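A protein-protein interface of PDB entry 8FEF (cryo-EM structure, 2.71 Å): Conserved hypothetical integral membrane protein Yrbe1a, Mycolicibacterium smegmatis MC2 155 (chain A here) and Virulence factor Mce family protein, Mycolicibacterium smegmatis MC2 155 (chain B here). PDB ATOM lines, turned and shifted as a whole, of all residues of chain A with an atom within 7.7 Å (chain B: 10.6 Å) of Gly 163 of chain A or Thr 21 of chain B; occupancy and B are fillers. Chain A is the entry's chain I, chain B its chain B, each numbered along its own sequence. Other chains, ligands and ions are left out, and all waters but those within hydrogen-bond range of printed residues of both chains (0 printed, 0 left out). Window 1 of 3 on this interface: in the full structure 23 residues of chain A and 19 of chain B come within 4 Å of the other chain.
OG of Ser 14 of chain B is in hydrogen-bond range of SD of Met 160 of chain A, 3.7 Å away.
The backbone carbonyl oxygen (O) of Leu 17 of chain B is in hydrogen-bond range of the side-chain hydroxyl (OG1) of Thr 21 of chain B. O of Gly 163 of chain A sits at hydrogen-bond distance from OG1 of Thr 167 of chain A (3.3 Å).
Among the printed residues, pairs that only touch across the chains: Phe 159 of chain A with Leu 18 of chain B (3.5 Å), Phe 159 of chain A with Thr 21 of chain B (3.7 Å), Met 160 of chain A with Phe 13 of chain B (3.97 Å), Met 160 of chain A with Leu 17 of chain B (3.7 Å), Gly 163 of chain A with Thr 21 of chain B (3.7 Å), Gly 163 of chain A with Ile 24 of chain B (3.2 Å), Ala 164 of chain A with Leu 17 of chain B (3.6 Å), Ile 166 of chain A with Ile 24 of chain B (3.7 Å), Thr 167 of chain A with Phe 20 of chain B (3.8 Å), Thr 167 of chain A with Ile 24 of chain B (3.3 Å), Leu 170 of chain A with Phe 28 of chain B (3.5 Å), Val 201 of chain A with Ile 24 of chain B (3.8 Å), Val 201 of chain A with Phe 25 of chain B (3.6 Å), Val 201 of chain A with Phe 28 of chain B (3.9 Å) and Val 205 of chain A with Phe 25 of chain B (3.7 Å).
Of the printed residues of chain B, Phe 159 of chain A touches Leu 18 (3.5 Å) and Thr 21 (3.7 Å). Printed residues of chain B within 4 Å of Met 160 of chain A: Phe 13 (3.97 Å), Ser 14 (3.7 Å) and Leu 17 (3.7 Å). No residue of chain B comes within 4 Å of Asn 162 of chain A. Gly 163 of chain A touches just these residues of chain B: Thr 21 and Ile 24. Ala 164 of chain A touches one residue of chain B. Val 165 of chain A touches none of the printed residues of chain B. Of chain B, only Ile 24 (3.7 Å) comes within 4 Å of Ile 166 of chain A. Ala 22 of chain B touches none of the printed residues of chain A. Printed residues of chain A within 4 Å of Phe 25 of chain B: Val 201 (3.6 Å) and Val 205 (3.7 Å). Val 26 of chain B touches none of the printed residues of chain A. Printed residues of chain A within 4 Å of Phe 28 of chain B: Leu 170 (3.5 Å) and Val 201 (3.9 Å). The nearest residue of chain A that does not touch Thr 21 of chain B is Met 160 of chain A (4.8 Å). The nearest printed residue of chain A that does not touch Leu 17 of chain B is Leu 161 of chain A (4.4 Å).
Of the 21 printed residues of chain A, 9 touch a printed residue of chain B. Hydrophobic or aromatic side chains of chain A within 4 Å of the printed part of chain B: Phe 159, Met 160, Ala 164, Ile 166, Leu 170, Val 201 and Val 205. Printed residues of chain B that touch a printed residue of chain A: Phe 13, Ser 14, Leu 17, Leu 18, Phe 20, Thr 21, Ile 24, Phe 25 and Phe 28. Hydrophobic or aromatic side chains of chain B that line the printed part of chain A: Leu 17, Leu 18, Phe 20, Ile 24, Phe 25 and Phe 28. Along chain B the printed residues that touch a printed residue of chain A span positions 13 to 28. Among the printed residues, no Asp or Glu carboxylate lies within 4 Å of a Lys or Arg side-chain nitrogen of the other chain.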
ATOM      1  N   GLY A 103       0.985   9.579   6.290  1.00  0.00           N
ATOM      2  CA  GLY A 103       0.519   8.998   5.054  1.00  0.00           C
ATOM      3  C   GLY A 103      -0.270   9.976   4.208  1.00  0.00           C
ATOM      4  O   GLY A 103       0.128  10.327   3.091  1.00  0.00           O
ATOM      5  N   PRO A 104      -1.424  10.419   4.720  1.00  0.00           N
ATOM      6  CA  PRO A 104      -2.234  11.389   3.967  1.00  0.00           C
ATOM      7  C   PRO A 104      -1.528  12.705   3.675  1.00  0.00           C
ATOM      8  O   PRO A 104      -1.778  13.291   2.620  1.00  0.00           O
ATOM      9  CB  PRO A 104      -3.458  11.589   4.870  1.00  0.00           C
ATOM     10  CG  PRO A 104      -3.572  10.316   5.612  1.00  0.00           C
ATOM     11  CD  PRO A 104      -2.163   9.876   5.874  1.00  0.00           C
ATOM     12  N   THR A 107       0.892  12.175   0.940  1.00  0.00           N
ATOM     13  CA  THR A 107       0.037  12.052  -0.234  1.00  0.00           C
ATOM     14  C   THR A 107      -0.394  13.422  -0.743  1.00  0.00           C
ATOM     15  O   THR A 107      -0.333  13.689  -1.945  1.00  0.00           O
ATOM     16  CB  THR A 107      -1.182  11.189   0.096  1.00  0.00           C
ATOM     17  OG1 THR A 107      -0.755   9.857   0.402  1.00  0.00           O
ATOM     18  CG2 THR A 107      -2.147  11.149  -1.078  1.00  0.00           C
ATOM     19  N   VAL A 157      -4.648   6.486  -7.654  1.00  0.00           N
ATOM     20  CA  VAL A 157      -3.229   6.644  -7.368  1.00  0.00           C
ATOM     21  C   VAL A 157      -3.022   7.176  -5.957  1.00  0.00           C
ATOM     22  O   VAL A 157      -2.095   6.754  -5.260  1.00  0.00           O
ATOM     23  CB  VAL A 157      -2.567   7.542  -8.428  1.00  0.00           C
ATOM     24  CG1 VAL A 157      -1.128   7.836  -8.060  1.00  0.00           C
ATOM     25  CG2 VAL A 157      -2.617   6.865  -9.783  1.00  0.00           C
ATOM     26  N   ALA A 158      -3.878   8.098  -5.503  1.00  0.00           N
ATOM     27  CA  ALA A 158      -3.754   8.600  -4.138  1.00  0.00           C
ATOM     28  C   ALA A 158      -3.965   7.487  -3.119  1.00  0.00           C
ATOM     29  O   ALA A 158      -3.229   7.397  -2.129  1.00  0.00           O
ATOM     30  CB  ALA A 158      -4.744   9.736  -3.900  1.00  0.00           C
ATOM     31  N   PHE A 159      -4.962   6.630  -3.351  1.00  0.00           N
ATOM     32  CA  PHE A 159      -5.203   5.488  -2.470  1.00  0.00           C
ATOM     33  C   PHE A 159      -3.967   4.593  -2.376  1.00  0.00           C
ATOM     34  O   PHE A 159      -3.467   4.296  -1.273  1.00  0.00           O
ATOM     35  CB  PHE A 159      -6.413   4.715  -3.000  1.00  0.00           C
ATOM     36  CG  PHE A 159      -6.827   3.542  -2.159  1.00  0.00           C
ATOM     37  CD1 PHE A 159      -7.739   3.699  -1.132  1.00  0.00           C
ATOM     38  CD2 PHE A 159      -6.341   2.273  -2.427  1.00  0.00           C
ATOM     39  CE1 PHE A 159      -8.133   2.621  -0.370  1.00  0.00           C
ATOM     40  CE2 PHE A 159      -6.734   1.194  -1.665  1.00  0.00           C
ATOM     41  CZ  PHE A 159      -7.631   1.368  -0.636  1.00  0.00           C
ATOM     42  N   MET A 160      -3.445   4.175  -3.535  1.00  0.00           N
ATOM     43  CA  MET A 160      -2.296   3.272  -3.542  1.00  0.00           C
ATOM     44  C   MET A 160      -1.064   3.924  -2.919  1.00  0.00           C
ATOM     45  O   MET A 160      -0.321   3.278  -2.164  1.00  0.00           O
ATOM     46  CB  MET A 160      -2.005   2.816  -4.969  1.00  0.00           C
ATOM     47  CG  MET A 160      -2.916   1.706  -5.453  1.00  0.00           C
ATOM     48  SD  MET A 160      -2.958   1.592  -7.246  1.00  0.00           S
ATOM     49  CE  MET A 160      -1.228   1.805  -7.640  1.00  0.00           C
ATOM     50  N   LEU A 161      -0.829   5.203  -3.223  1.00  0.00           N
ATOM     51  CA  LEU A 161       0.339   5.893  -2.694  1.00  0.00           C
ATOM     52  C   LEU A 161       0.244   6.072  -1.188  1.00  0.00           C
ATOM     53  O   LEU A 161       1.258   5.989  -0.493  1.00  0.00           O
ATOM     54  CB  LEU A 161       0.519   7.244  -3.386  1.00  0.00           C
ATOM     55  CG  LEU A 161       1.011   7.207  -4.832  1.00  0.00           C
ATOM     56  CD1 LEU A 161       1.270   8.615  -5.329  1.00  0.00           C
ATOM     57  CD2 LEU A 161       2.257   6.346  -4.961  1.00  0.00           C
ATOM     58  N   ASN A 162      -0.956   6.328  -0.662  1.00  0.00           N
ATOM     59  CA  ASN A 162      -1.117   6.422   0.785  1.00  0.00           C
ATOM     60  C   ASN A 162      -0.775   5.100   1.457  1.00  0.00           C
ATOM     61  O   ASN A 162      -0.069   5.072   2.477  1.00  0.00           O
ATOM     62  CB  ASN A 162      -2.544   6.838   1.127  1.00  0.00           C
ATOM     63  CG  ASN A 162      -2.815   6.814   2.613  1.00  0.00           C
ATOM     64  OD1 ASN A 162      -1.951   7.156   3.418  1.00  0.00           O
ATOM     65  ND2 ASN A 162      -4.017   6.400   2.987  1.00  0.00           N
ATOM     66  N   GLY A 163      -1.270   3.992   0.898  1.00  0.00           N
ATOM     67  CA  GLY A 163      -0.916   2.692   1.455  1.00  0.00           C
ATOM     68  C   GLY A 163       0.584   2.452   1.454  1.00  0.00           C
ATOM     69  O   GLY A 163       1.170   2.038   2.467  1.00  0.00           O
ATOM     70  N   ALA A 164       1.230   2.735   0.319  1.00  0.00           N
ATOM     71  CA  ALA A 164       2.672   2.527   0.212  1.00  0.00           C
ATOM     72  C   ALA A 164       3.439   3.424   1.175  1.00  0.00           C
ATOM     73  O   ALA A 164       4.435   2.995   1.769  1.00  0.00           O
ATOM     74  CB  ALA A 164       3.133   2.774  -1.223  1.00  0.00           C
ATOM     75  N   VAL A 165       2.998   4.674   1.334  1.00  0.00           N
ATOM     76  CA  VAL A 165       3.674   5.605   2.234  1.00  0.00           C
ATOM     77  C   VAL A 165       3.599   5.109   3.669  1.00  0.00           C
ATOM     78  O   VAL A 165       4.597   5.125   4.396  1.00  0.00           O
ATOM     79  CB  VAL A 165       3.080   7.019   2.097  1.00  0.00           C
ATOM     80  CG1 VAL A 165       3.465   7.877   3.285  1.00  0.00           C
ATOM     81  CG2 VAL A 165       3.576   7.666   0.837  1.00  0.00           C
ATOM     82  N   ILE A 166       2.417   4.662   4.100  1.00  0.00           N
ATOM     83  CA  ILE A 166       2.281   4.175   5.472  1.00  0.00           C
ATOM     84  C   ILE A 166       3.183   2.966   5.702  1.00  0.00           C
ATOM     85  O   ILE A 166       3.906   2.890   6.707  1.00  0.00           O
ATOM     86  CB  ILE A 166       0.809   3.859   5.793  1.00  0.00           C
ATOM     87  CG1 ILE A 166      -0.038   5.126   5.693  1.00  0.00           C
ATOM     88  CG2 ILE A 166       0.686   3.258   7.181  1.00  0.00           C
ATOM     89  CD1 ILE A 166      -1.496   4.907   6.004  1.00  0.00           C
ATOM     90  N   THR A 167       3.175   2.012   4.761  1.00  0.00           N
ATOM     91  CA  THR A 167       3.996   0.812   4.929  1.00  0.00           C
ATOM     92  C   THR A 167       5.484   1.152   4.980  1.00  0.00           C
ATOM     93  O   THR A 167       6.213   0.693   5.873  1.00  0.00           O
ATOM     94  CB  THR A 167       3.715  -0.182   3.802  1.00  0.00           C
ATOM     95  OG1 THR A 167       2.387  -0.697   3.938  1.00  0.00           O
ATOM     96  CG2 THR A 167       4.703  -1.336   3.848  1.00  0.00           C
ATOM     97  N   ILE A 168       5.949   1.968   4.029  1.00  0.00           N
ATOM     98  CA  ILE A 168       7.367   2.311   3.953  1.00  0.00           C
ATOM     99  C   ILE A 168       7.787   3.107   5.181  1.00  0.00           C
ATOM    100  O   ILE A 168       8.879   2.902   5.724  1.00  0.00           O
ATOM    101  CB  ILE A 168       7.662   3.065   2.638  1.00  0.00           C
ATOM    102  CG1 ILE A 168       8.120   2.093   1.544  1.00  0.00           C
ATOM    103  CG2 ILE A 168       8.705   4.159   2.837  1.00  0.00           C
ATOM    104  CD1 ILE A 168       7.076   1.087   1.102  1.00  0.00           C
ATOM    105  N   GLY A 169       6.923   4.012   5.651  1.00  0.00           N
ATOM    106  CA  GLY A 169       7.239   4.771   6.846  1.00  0.00           C
ATOM    107  C   GLY A 169       7.386   3.896   8.073  1.00  0.00           C
ATOM    108  O   GLY A 169       8.328   4.062   8.851  1.00  0.00           O
ATOM    109  N   LEU A 170       6.462   2.948   8.262  1.00  0.00           N
ATOM    110  CA  LEU A 170       6.560   2.051   9.411  1.00  0.00           C
ATOM    111  C   LEU A 170       7.830   1.209   9.352  1.00  0.00           C
ATOM    112  O   LEU A 170       8.543   1.069  10.354  1.00  0.00           O
ATOM    113  CB  LEU A 170       5.327   1.153   9.483  1.00  0.00           C
ATOM    114  CG  LEU A 170       4.006   1.824   9.846  1.00  0.00           C
ATOM    115  CD1 LEU A 170       2.902   0.795   9.826  1.00  0.00           C
ATOM    116  CD2 LEU A 170       4.093   2.495  11.204  1.00  0.00           C
ATOM    117  N   VAL A 201      -7.006   3.300  10.175  1.00  0.00           N
ATOM    118  CA  VAL A 201      -6.764   2.952   8.777  1.00  0.00           C
ATOM    119  C   VAL A 201      -7.947   3.363   7.907  1.00  0.00           C
ATOM    120  O   VAL A 201      -7.761   3.788   6.760  1.00  0.00           O
ATOM    121  CB  VAL A 201      -6.421   1.455   8.628  1.00  0.00           C
ATOM    122  CG1 VAL A 201      -5.119   1.143   9.343  1.00  0.00           C
ATOM    123  CG2 VAL A 201      -7.528   0.577   9.163  1.00  0.00           C
ATOM    124  N   SER A 204      -7.717   7.086   7.392  1.00  0.00           N
ATOM    125  CA  SER A 204      -6.611   7.328   6.472  1.00  0.00           C
ATOM    126  C   SER A 204      -7.022   7.059   5.030  1.00  0.00           C
ATOM    127  O   SER A 204      -6.685   7.831   4.124  1.00  0.00           O
ATOM    128  CB  SER A 204      -5.420   6.457   6.859  1.00  0.00           C
ATOM    129  OG  SER A 204      -4.330   6.664   5.980  1.00  0.00           O
ATOM    130  N   VAL A 205      -7.747   5.962   4.801  1.00  0.00           N
ATOM    131  CA  VAL A 205      -8.227   5.638   3.460  1.00  0.00           C
ATOM    132  C   VAL A 205      -9.177   6.717   2.956  1.00  0.00           C
ATOM    133  O   VAL A 205      -9.096   7.149   1.797  1.00  0.00           O
ATOM    134  CB  VAL A 205      -8.889   4.247   3.467  1.00  0.00           C
ATOM    135  CG1 VAL A 205      -9.836   4.087   2.291  1.00  0.00           C
ATOM    136  CG2 VAL A 205      -7.830   3.159   3.450  1.00  0.00           C
ATOM    137  N   ALA A 208      -7.166   9.812   2.007  1.00  0.00           N
ATOM    138  CA  ALA A 208      -6.450   9.653   0.744  1.00  0.00           C
ATOM    139  C   ALA A 208      -7.393   9.749  -0.448  1.00  0.00           C
ATOM    140  O   ALA A 208      -7.079  10.410  -1.447  1.00  0.00           O
ATOM    141  CB  ALA A 208      -5.713   8.320   0.727  1.00  0.00           C
ATOM    142  N   PHE B  13       1.727  -2.763 -10.761  1.00  0.00           N
ATOM    143  CA  PHE B  13       1.916  -1.749  -9.727  1.00  0.00           C
ATOM    144  C   PHE B  13       0.713  -1.683  -8.794  1.00  0.00           C
ATOM    145  O   PHE B  13       0.868  -1.569  -7.570  1.00  0.00           O
ATOM    146  CB  PHE B  13       2.167  -0.389 -10.377  1.00  0.00           C
ATOM    147  CG  PHE B  13       3.261   0.400  -9.725  1.00  0.00           C
ATOM    148  CD1 PHE B  13       4.579   0.221 -10.104  1.00  0.00           C
ATOM    149  CD2 PHE B  13       2.972   1.322  -8.734  1.00  0.00           C
ATOM    150  CE1 PHE B  13       5.590   0.946  -9.508  1.00  0.00           C
ATOM    151  CE2 PHE B  13       3.978   2.049  -8.133  1.00  0.00           C
ATOM    152  CZ  PHE B  13       5.290   1.861  -8.521  1.00  0.00           C
ATOM    153  N   SER B  14      -0.494  -1.767  -9.357  1.00  0.00           N
ATOM    154  CA  SER B  14      -1.708  -1.742  -8.557  1.00  0.00           C
ATOM    155  C   SER B  14      -1.792  -2.962  -7.657  1.00  0.00           C
ATOM    156  O   SER B  14      -2.199  -2.851  -6.500  1.00  0.00           O
ATOM    157  CB  SER B  14      -2.933  -1.657  -9.466  1.00  0.00           C
ATOM    158  OG  SER B  14      -2.893  -0.485 -10.259  1.00  0.00           O
ATOM    159  N   LEU B  15      -1.414  -4.134  -8.170  1.00  0.00           N
ATOM    160  CA  LEU B  15      -1.409  -5.337  -7.347  1.00  0.00           C
ATOM    161  C   LEU B  15      -0.468  -5.181  -6.159  1.00  0.00           C
ATOM    162  O   LEU B  15      -0.839  -5.487  -5.022  1.00  0.00           O
ATOM    163  CB  LEU B  15      -1.016  -6.546  -8.194  1.00  0.00           C
ATOM    164  CG  LEU B  15      -1.342  -7.921  -7.613  1.00  0.00           C
ATOM    165  CD1 LEU B  15      -2.838  -8.175  -7.670  1.00  0.00           C
ATOM    166  CD2 LEU B  15      -0.578  -9.007  -8.348  1.00  0.00           C
ATOM    167  N   VAL B  16       0.753  -4.696  -6.403  1.00  0.00           N
ATOM    168  CA  VAL B  16       1.718  -4.547  -5.312  1.00  0.00           C
ATOM    169  C   VAL B  16       1.228  -3.534  -4.276  1.00  0.00           C
ATOM    170  O   VAL B  16       1.279  -3.781  -3.059  1.00  0.00           O
ATOM    171  CB  VAL B  16       3.099  -4.161  -5.871  1.00  0.00           C
ATOM    172  CG1 VAL B  16       4.069  -3.879  -4.738  1.00  0.00           C
ATOM    173  CG2 VAL B  16       3.634  -5.264  -6.764  1.00  0.00           C
ATOM    174  N   LEU B  17       0.693  -2.400  -4.735  1.00  0.00           N
ATOM    175  CA  LEU B  17       0.323  -1.369  -3.774  1.00  0.00           C
ATOM    176  C   LEU B  17      -0.986  -1.692  -3.063  1.00  0.00           C
ATOM    177  O   LEU B  17      -1.169  -1.317  -1.895  1.00  0.00           O
ATOM    178  CB  LEU B  17       0.249  -0.014  -4.476  1.00  0.00           C
ATOM    179  CG  LEU B  17       1.616   0.531  -4.911  1.00  0.00           C
ATOM    180  CD1 LEU B  17       1.548   2.005  -5.278  1.00  0.00           C
ATOM    181  CD2 LEU B  17       2.681   0.288  -3.852  1.00  0.00           C
ATOM    182  N   LEU B  18      -1.874  -2.459  -3.699  1.00  0.00           N
ATOM    183  CA  LEU B  18      -3.048  -2.899  -2.969  1.00  0.00           C
ATOM    184  C   LEU B  18      -2.691  -4.028  -2.021  1.00  0.00           C
ATOM    185  O   LEU B  18      -3.357  -4.194  -0.996  1.00  0.00           O
ATOM    186  CB  LEU B  18      -4.143  -3.344  -3.940  1.00  0.00           C
ATOM    187  CG  LEU B  18      -4.805  -2.257  -4.790  1.00  0.00           C
ATOM    188  CD1 LEU B  18      -5.800  -2.871  -5.761  1.00  0.00           C
ATOM    189  CD2 LEU B  18      -5.479  -1.220  -3.916  1.00  0.00           C
ATOM    190  N   THR B  19      -1.661  -4.819  -2.345  1.00  0.00           N
ATOM    191  CA  THR B  19      -1.149  -5.777  -1.376  1.00  0.00           C
ATOM    192  C   THR B  19      -0.656  -5.052  -0.134  1.00  0.00           C
ATOM    193  O   THR B  19      -0.876  -5.509   0.992  1.00  0.00           O
ATOM    194  CB  THR B  19      -0.033  -6.615  -2.001  1.00  0.00           C
ATOM    195  OG1 THR B  19      -0.558  -7.363  -3.103  1.00  0.00           O
ATOM    196  CG2 THR B  19       0.556  -7.577  -0.983  1.00  0.00           C
ATOM    197  N   PHE B  20      -0.019  -3.891  -0.325  1.00  0.00           N
ATOM    198  CA  PHE B  20       0.440  -3.112   0.826  1.00  0.00           C
ATOM    199  C   PHE B  20      -0.731  -2.563   1.637  1.00  0.00           C
ATOM    200  O   PHE B  20      -0.702  -2.586   2.874  1.00  0.00           O
ATOM    201  CB  PHE B  20       1.357  -1.972   0.382  1.00  0.00           C
ATOM    202  CG  PHE B  20       2.735  -2.418  -0.008  1.00  0.00           C
ATOM    203  CD1 PHE B  20       3.223  -3.645   0.402  1.00  0.00           C
ATOM    204  CD2 PHE B  20       3.551  -1.598  -0.768  1.00  0.00           C
ATOM    205  CE1 PHE B  20       4.493  -4.054   0.050  1.00  0.00           C
ATOM    206  CE2 PHE B  20       4.822  -2.001  -1.123  1.00  0.00           C
ATOM    207  CZ  PHE B  20       5.294  -3.231  -0.714  1.00  0.00           C
ATOM    208  N   THR B  21      -1.773  -2.076   0.959  1.00  0.00           N
ATOM    209  CA  THR B  21      -2.947  -1.575   1.678  1.00  0.00           C
ATOM    210  C   THR B  21      -3.658  -2.694   2.442  1.00  0.00           C
ATOM    211  O   THR B  21      -4.058  -2.516   3.603  1.00  0.00           O
ATOM    212  CB  THR B  21      -3.909  -0.895   0.706  1.00  0.00           C
ATOM    213  OG1 THR B  21      -3.229   0.166   0.023  1.00  0.00           O
ATOM    214  CG2 THR B  21      -5.102  -0.318   1.449  1.00  0.00           C
ATOM    215  N   ALA B  22      -3.811  -3.859   1.808  1.00  0.00           N
ATOM    216  CA  ALA B  22      -4.402  -5.014   2.476  1.00  0.00           C
ATOM    217  C   ALA B  22      -3.552  -5.465   3.655  1.00  0.00           C
ATOM    218  O   ALA B  22      -4.086  -5.876   4.691  1.00  0.00           O
ATOM    219  CB  ALA B  22      -4.591  -6.157   1.480  1.00  0.00           C
ATOM    220  N   LEU B  23      -2.227  -5.414   3.511  1.00  0.00           N
ATOM    221  CA  LEU B  23      -1.341  -5.774   4.611  1.00  0.00           C
ATOM    222  C   LEU B  23      -1.507  -4.815   5.781  1.00  0.00           C
ATOM    223  O   LEU B  23      -1.492  -5.236   6.941  1.00  0.00           O
ATOM    224  CB  LEU B  23       0.108  -5.797   4.119  1.00  0.00           C
ATOM    225  CG  LEU B  23       1.238  -6.101   5.103  1.00  0.00           C
ATOM    226  CD1 LEU B  23       2.266  -6.990   4.435  1.00  0.00           C
ATOM    227  CD2 LEU B  23       1.896  -4.821   5.587  1.00  0.00           C
ATOM    228  N   ILE B  24      -1.664  -3.521   5.494  1.00  0.00           N
ATOM    229  CA  ILE B  24      -1.909  -2.553   6.561  1.00  0.00           C
ATOM    230  C   ILE B  24      -3.222  -2.863   7.269  1.00  0.00           C
ATOM    231  O   ILE B  24      -3.303  -2.827   8.506  1.00  0.00           O
ATOM    232  CB  ILE B  24      -1.904  -1.120   5.997  1.00  0.00           C
ATOM    233  CG1 ILE B  24      -0.502  -0.722   5.551  1.00  0.00           C
ATOM    234  CG2 ILE B  24      -2.432  -0.128   7.022  1.00  0.00           C
ATOM    235  CD1 ILE B  24      -0.478   0.582   4.814  1.00  0.00           C
ATOM    236  N   PHE B  25      -4.267  -3.177   6.497  1.00  0.00           N
ATOM    237  CA  PHE B  25      -5.553  -3.520   7.101  1.00  0.00           C
ATOM    238  C   PHE B  25      -5.454  -4.775   7.964  1.00  0.00           C
ATOM    239  O   PHE B  25      -6.028  -4.828   9.056  1.00  0.00           O
ATOM    240  CB  PHE B  25      -6.618  -3.699   6.019  1.00  0.00           C
ATOM    241  CG  PHE B  25      -7.341  -2.432   5.667  1.00  0.00           C
ATOM    242  CD1 PHE B  25      -8.351  -1.949   6.481  1.00  0.00           C
ATOM    243  CD2 PHE B  25      -7.015  -1.726   4.523  1.00  0.00           C
ATOM    244  CE1 PHE B  25      -9.021  -0.783   6.161  1.00  0.00           C
ATOM    245  CE2 PHE B  25      -7.681  -0.560   4.199  1.00  0.00           C
ATOM    246  CZ  PHE B  25      -8.685  -0.090   5.019  1.00  0.00           C
ATOM    247  N   VAL B  26      -4.727  -5.789   7.493  1.00  0.00           N
ATOM    248  CA  VAL B  26      -4.560  -7.019   8.264  1.00  0.00           C
ATOM    249  C   VAL B  26      -3.778  -6.751   9.546  1.00  0.00           C
ATOM    250  O   VAL B  26      -4.131  -7.256  10.619  1.00  0.00           O
ATOM    251  CB  VAL B  26      -3.886  -8.102   7.400  1.00  0.00           C
ATOM    252  CG1 VAL B  26      -3.439  -9.273   8.253  1.00  0.00           C
ATOM    253  CG2 VAL B  26      -4.840  -8.579   6.320  1.00  0.00           C
ATOM    254  N   VAL B  27      -2.713  -5.953   9.460  1.00  0.00           N
ATOM    255  CA  VAL B  27      -1.854  -5.724  10.619  1.00  0.00           C
ATOM    256  C   VAL B  27      -2.586  -4.914  11.682  1.00  0.00           C
ATOM    257  O   VAL B  27      -2.568  -5.263  12.868  1.00  0.00           O
ATOM    258  CB  VAL B  27      -0.542  -5.043  10.189  1.00  0.00           C
ATOM    259  CG1 VAL B  27       0.171  -4.453  11.388  1.00  0.00           C
ATOM    260  CG2 VAL B  27       0.360  -6.042   9.488  1.00  0.00           C
ATOM    261  N   PHE B  28      -3.251  -3.834  11.283  1.00  0.00           N
ATOM    262  CA  PHE B  28      -3.878  -2.959  12.266  1.00  0.00           C
ATOM    263  C   PHE B  28      -5.322  -3.329  12.574  1.00  0.00           C
ATOM    264  O   PHE B  28      -5.925  -2.711  13.456  1.00  0.00           O
ATOM    265  CB  PHE B  28      -3.792  -1.503  11.808  1.00  0.00           C
ATOM    266  CG  PHE B  28      -2.398  -0.960  11.824  1.00  0.00           C
ATOM    267  CD1 PHE B  28      -1.801  -0.605  13.020  1.00  0.00           C
ATOM    268  CD2 PHE B  28      -1.678  -0.822  10.654  1.00  0.00           C
ATOM    269  CE1 PHE B  28      -0.518  -0.114  13.048  1.00  0.00           C
ATOM    270  CE2 PHE B  28      -0.393  -0.330  10.677  1.00  0.00           C
ATOM    271  CZ  PHE B  28       0.187   0.023  11.879  1.00  0.00           C
ATOM    272  N   GLY B  29      -5.887  -4.316  11.888  1.00  0.00           N
ATOM    273  CA  GLY B  29      -7.224  -4.774  12.177  1.00  0.00           C
ATOM    274  C   GLY B  29      -7.280  -6.075  12.936  1.00  0.00           C
ATOM    275  O   GLY B  29      -8.373  -6.509  13.310  1.00  0.00           O
ATOM    276  N   ILE B  31      -6.522  -9.369  11.993  1.00  0.00           N
ATOM    277  CA  ILE B  31      -7.237 -10.356  11.193  1.00  0.00           C
ATOM    278  C   ILE B  31      -6.512 -11.689  11.300  1.00  0.00           C
ATOM    279  O   ILE B  31      -5.293 -11.757  11.094  1.00  0.00           O
ATOM    280  CB  ILE B  31      -7.352  -9.908   9.726  1.00  0.00           C
ATOM    281  CG1 ILE B  31      -7.939  -8.499   9.639  1.00  0.00           C
ATOM    282  CG2 ILE B  31      -8.206 -10.879   8.936  1.00  0.00           C
ATOM    283  CD1 ILE B  31      -9.340  -8.385  10.176  1.00  0.00           C
